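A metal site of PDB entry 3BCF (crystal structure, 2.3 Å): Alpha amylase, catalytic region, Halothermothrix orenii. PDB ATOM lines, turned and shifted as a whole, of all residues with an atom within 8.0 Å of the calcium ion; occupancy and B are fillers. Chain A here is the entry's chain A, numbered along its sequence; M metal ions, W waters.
The nearest printed residue that does not touch the calcium ion is Met 421 (4.1 Å).
O of Asp 518 lies within hydrogen-bond range of OG of Ser 540 (2.8 Å). OD1 of Asp 516 lies within hydrogen-bond range of N of Asp 518 (2.8 Å). O of Asp 541 is in hydrogen-bond range of NH2 of Arg 462. The backbone carbonyl oxygen (O) of Ala 517 lies close to the backbone NH (N) of Met 421.
The calcium ion is bound by water W1 (2.2 Å), the backbone carbonyl oxygen (O) of Ala 517 (2.3 Å), the side-chain carboxylate (OD1) of Asp 518 (2.3 Å), the backbone carbonyl oxygen (O) of Ala 419 (2.3 Å), the side-chain carboxylate (OD1) of Asp 541 (2.4 Å) and the side-chain carboxylate (OD2) of Asp 541 (2.4 Å). The calcium ion has six donor atoms within binding distance.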
ATOM      1  N   PHE A 411      23.757  21.372  -0.256  1.00  0.00           N
ATOM      2  CA  PHE A 411      24.157  20.027  -0.476  1.00  0.00           C
ATOM      3  C   PHE A 411      25.644  19.898  -0.826  1.00  0.00           C
ATOM      4  O   PHE A 411      26.323  18.989  -0.331  1.00  0.00           O
ATOM      5  CB  PHE A 411      23.310  19.296  -1.529  1.00  0.00           C
ATOM      6  CG  PHE A 411      23.458  17.798  -1.462  1.00  0.00           C
ATOM      7  CD1 PHE A 411      22.560  17.032  -0.765  1.00  0.00           C
ATOM      8  CD2 PHE A 411      24.577  17.173  -1.989  1.00  0.00           C
ATOM      9  CE1 PHE A 411      22.730  15.612  -0.638  1.00  0.00           C
ATOM     10  CE2 PHE A 411      24.754  15.764  -1.892  1.00  0.00           C
ATOM     11  CZ  PHE A 411      23.831  15.000  -1.207  1.00  0.00           C
ATOM     12  N   ASP A 414      27.539  20.076   2.166  1.00  0.00           N
ATOM     13  CA  ASP A 414      27.405  18.798   2.913  1.00  0.00           C
ATOM     14  C   ASP A 414      28.467  17.783   2.390  1.00  0.00           C
ATOM     15  O   ASP A 414      29.203  17.196   3.120  1.00  0.00           O
ATOM     16  CB  ASP A 414      25.951  18.312   2.773  1.00  0.00           C
ATOM     17  CG  ASP A 414      25.622  17.027   3.529  1.00  0.00           C
ATOM     18  OD1 ASP A 414      26.424  16.521   4.387  1.00  0.00           O
ATOM     19  OD2 ASP A 414      24.481  16.530   3.243  1.00  0.00           O
ATOM     20  N   MET A 415      28.600  17.705   1.086  1.00  0.00           N
ATOM     21  CA  MET A 415      29.644  16.934   0.470  1.00  0.00           C
ATOM     22  C   MET A 415      31.077  17.322   0.857  1.00  0.00           C
ATOM     23  O   MET A 415      31.969  16.543   0.629  1.00  0.00           O
ATOM     24  CB  MET A 415      29.516  17.031  -1.032  1.00  0.00           C
ATOM     25  CG  MET A 415      28.333  16.331  -1.661  1.00  0.00           C
ATOM     26  SD  MET A 415      28.382  16.618  -3.471  1.00  0.00           S
ATOM     27  CE  MET A 415      30.090  16.156  -3.810  1.00  0.00           C
ATOM     28  N   ASN A 417      32.655  17.203   3.734  1.00  0.00           N
ATOM     29  CA  ASN A 417      33.118  16.044   4.495  1.00  0.00           C
ATOM     30  C   ASN A 417      32.327  14.728   4.271  1.00  0.00           C
ATOM     31  O   ASN A 417      32.259  13.953   5.151  1.00  0.00           O
ATOM     32  CB  ASN A 417      33.082  16.406   5.968  1.00  0.00           C
ATOM     33  CG  ASN A 417      31.690  16.827   6.430  1.00  0.00           C
ATOM     34  OD1 ASN A 417      30.700  16.686   5.691  1.00  0.00           O
ATOM     35  ND2 ASN A 417      31.622  17.313   7.669  1.00  0.00           N
ATOM     36  N   GLY A 418      31.762  14.496   3.099  1.00  0.00           N
ATOM     37  CA  GLY A 418      30.912  13.335   2.838  1.00  0.00           C
ATOM     38  C   GLY A 418      29.427  13.625   3.126  1.00  0.00           C
ATOM     39  O   GLY A 418      29.113  14.188   4.157  1.00  0.00           O
ATOM     40  N   ALA A 419      28.557  13.218   2.186  1.00  0.00           N
ATOM     41  CA  ALA A 419      27.122  13.423   2.166  1.00  0.00           C
ATOM     42  C   ALA A 419      26.490  12.088   1.771  1.00  0.00           C
ATOM     43  O   ALA A 419      27.187  11.192   1.352  1.00  0.00           O
ATOM     44  CB  ALA A 419      26.744  14.470   1.087  1.00  0.00           C
ATOM     45  N   TYR A 420      25.169  11.981   1.881  1.00  0.00           N
ATOM     46  CA  TYR A 420      24.433  10.825   1.384  1.00  0.00           C
ATOM     47  C   TYR A 420      24.041  11.101  -0.065  1.00  0.00           C
ATOM     48  O   TYR A 420      23.065  11.806  -0.363  1.00  0.00           O
ATOM     49  CB  TYR A 420      23.239  10.532   2.260  1.00  0.00           C
ATOM     50  CG  TYR A 420      22.778   9.119   2.113  1.00  0.00           C
ATOM     51  CD1 TYR A 420      23.338   8.081   2.855  1.00  0.00           C
ATOM     52  CD2 TYR A 420      21.774   8.810   1.212  1.00  0.00           C
ATOM     53  CE1 TYR A 420      22.906   6.756   2.693  1.00  0.00           C
ATOM     54  CE2 TYR A 420      21.355   7.519   1.028  1.00  0.00           C
ATOM     55  CZ  TYR A 420      21.919   6.496   1.763  1.00  0.00           C
ATOM     56  OH  TYR A 420      21.433   5.240   1.528  1.00  0.00           O
ATOM     57  N   MET A 421      24.839  10.583  -0.994  1.00  0.00           N
ATOM     58  CA  MET A 421      24.775  11.062  -2.362  1.00  0.00           C
ATOM     59  C   MET A 421      23.457  10.793  -3.112  1.00  0.00           C
ATOM     60  O   MET A 421      23.154  11.530  -4.080  1.00  0.00           O
ATOM     61  CB  MET A 421      25.977  10.578  -3.175  1.00  0.00           C
ATOM     62  CG  MET A 421      27.290  11.157  -2.704  1.00  0.00           C
ATOM     63  SD  MET A 421      27.480  12.859  -3.094  1.00  0.00           S
ATOM     64  CE  MET A 421      27.727  12.773  -4.866  1.00  0.00           C
ATOM     65  N   ALA A 422      22.680   9.814  -2.675  1.00  0.00           N
ATOM     66  CA  ALA A 422      21.415   9.519  -3.299  1.00  0.00           C
ATOM     67  C   ALA A 422      20.453  10.657  -3.125  1.00  0.00           C
ATOM     68  O   ALA A 422      19.511  10.780  -3.896  1.00  0.00           O
ATOM     69  CB  ALA A 422      20.781   8.228  -2.772  1.00  0.00           C
ATOM     70  N   ARG A 462      35.656  18.594  -3.991  1.00  0.00           N
ATOM     71  CA  ARG A 462      34.569  18.047  -4.852  1.00  0.00           C
ATOM     72  C   ARG A 462      33.813  19.071  -5.756  1.00  0.00           C
ATOM     73  O   ARG A 462      32.702  18.866  -6.204  1.00  0.00           O
ATOM     74  CB  ARG A 462      33.609  17.191  -4.043  1.00  0.00           C
ATOM     75  CG  ARG A 462      34.334  16.046  -3.417  1.00  0.00           C
ATOM     76  CD  ARG A 462      33.406  15.131  -2.773  1.00  0.00           C
ATOM     77  NE  ARG A 462      34.084  14.027  -2.096  1.00  0.00           N
ATOM     78  CZ  ARG A 462      34.586  14.046  -0.857  1.00  0.00           C
ATOM     79  NH1 ARG A 462      34.583  15.143  -0.107  1.00  0.00           N
ATOM     80  NH2 ARG A 462      35.140  12.934  -0.406  1.00  0.00           N
ATOM     81  N   ASP A 516      23.433   5.509  -3.764  1.00  0.00           N
ATOM     82  CA  ASP A 516      23.736   5.084  -2.422  1.00  0.00           C
ATOM     83  C   ASP A 516      24.416   6.229  -1.693  1.00  0.00           C
ATOM     84  O   ASP A 516      24.294   7.419  -2.109  1.00  0.00           O
ATOM     85  CB  ASP A 516      24.559   3.760  -2.439  1.00  0.00           C
ATOM     86  CG  ASP A 516      25.903   3.875  -3.210  1.00  0.00           C
ATOM     87  OD1 ASP A 516      26.558   4.952  -3.169  1.00  0.00           O
ATOM     88  OD2 ASP A 516      26.303   2.862  -3.840  1.00  0.00           O
ATOM     89  N   ALA A 517      25.048   5.910  -0.559  1.00  0.00           N
ATOM     90  CA  ALA A 517      25.687   6.906   0.293  1.00  0.00           C
ATOM     91  C   ALA A 517      26.790   7.648  -0.449  1.00  0.00           C
ATOM     92  O   ALA A 517      27.076   8.821  -0.173  1.00  0.00           O
ATOM     93  CB  ALA A 517      26.228   6.257   1.550  1.00  0.00           C
ATOM     94  N   ASP A 518      27.428   6.934  -1.382  1.00  0.00           N
ATOM     95  CA  ASP A 518      28.585   7.505  -2.080  1.00  0.00           C
ATOM     96  C   ASP A 518      28.475   7.744  -3.570  1.00  0.00           C
ATOM     97  O   ASP A 518      29.282   8.498  -4.077  1.00  0.00           O
ATOM     98  CB  ASP A 518      29.872   6.758  -1.741  1.00  0.00           C
ATOM     99  CG  ASP A 518      30.116   6.679  -0.243  1.00  0.00           C
ATOM    100  OD1 ASP A 518      29.568   7.494   0.480  1.00  0.00           O
ATOM    101  OD2 ASP A 518      30.815   5.767   0.227  1.00  0.00           O
ATOM    102  N   ILE A 519      27.475   7.168  -4.277  1.00  0.00           N
ATOM    103  CA  ILE A 519      27.336   7.365  -5.733  1.00  0.00           C
ATOM    104  C   ILE A 519      25.991   7.901  -6.151  1.00  0.00           C
ATOM    105  O   ILE A 519      24.987   7.418  -5.712  1.00  0.00           O
ATOM    106  CB  ILE A 519      27.560   6.071  -6.516  1.00  0.00           C
ATOM    107  CG1 ILE A 519      29.015   5.600  -6.395  1.00  0.00           C
ATOM    108  CG2 ILE A 519      27.262   6.293  -8.017  1.00  0.00           C
ATOM    109  CD1 ILE A 519      29.230   4.100  -6.830  1.00  0.00           C
ATOM    110  N   SER A 540      30.751  10.883  -7.289  1.00  0.00           N
ATOM    111  CA  SER A 540      30.963  10.181  -6.066  1.00  0.00           C
ATOM    112  C   SER A 540      31.685  11.027  -5.081  1.00  0.00           C
ATOM    113  O   SER A 540      32.532  11.812  -5.414  1.00  0.00           O
ATOM    114  CB  SER A 540      31.742   8.872  -6.320  1.00  0.00           C
ATOM    115  OG  SER A 540      31.827   8.106  -5.119  1.00  0.00           O
ATOM    116  N   ASP A 541      31.330  10.858  -3.823  1.00  0.00           N
ATOM    117  CA  ASP A 541      32.118  11.425  -2.738  1.00  0.00           C
ATOM    118  C   ASP A 541      32.951  10.347  -2.066  1.00  0.00           C
ATOM    119  O   ASP A 541      33.527  10.574  -1.038  1.00  0.00           O
ATOM    120  CB  ASP A 541      31.245  12.171  -1.729  1.00  0.00           C
ATOM    121  CG  ASP A 541      30.352  11.270  -0.904  1.00  0.00           C
ATOM    122  OD1 ASP A 541      29.724  11.790   0.035  1.00  0.00           O
ATOM    123  OD2 ASP A 541      30.252  10.062  -1.157  1.00  0.00           O
ATOM    124  N   GLY A 542      33.055   9.198  -2.693  1.00  0.00           N
ATOM    125  CA  GLY A 542      33.931   8.159  -2.163  1.00  0.00           C
ATOM    126  C   GLY A 542      35.402   8.544  -2.238  1.00  0.00           C
ATOM    127  O   GLY A 542      35.779   9.416  -3.007  1.00  0.00           O
ATOM    128  N   THR A 543      36.190   7.864  -1.417  1.00  0.00           N
ATOM    129  CA  THR A 543      37.612   8.095  -1.213  1.00  0.00           C
ATOM    130  C   THR A 543      38.449   6.808  -1.284  1.00  0.00           C
ATOM    131  O   THR A 543      39.660   6.879  -1.184  1.00  0.00           O
ATOM    132  CB  THR A 543      37.845   8.759   0.158  1.00  0.00           C
ATOM    133  OG1 THR A 543      37.164   8.004   1.177  1.00  0.00           O
ATOM    134  CG2 THR A 543      37.328  10.237   0.156  1.00  0.00           C
HETATM  135 CA    CA M   1      28.926   9.718   0.807  1.00  0.00          CA
HETATM  136  O   HOH W   1      30.706  10.050   2.120  1.00  0.00           O
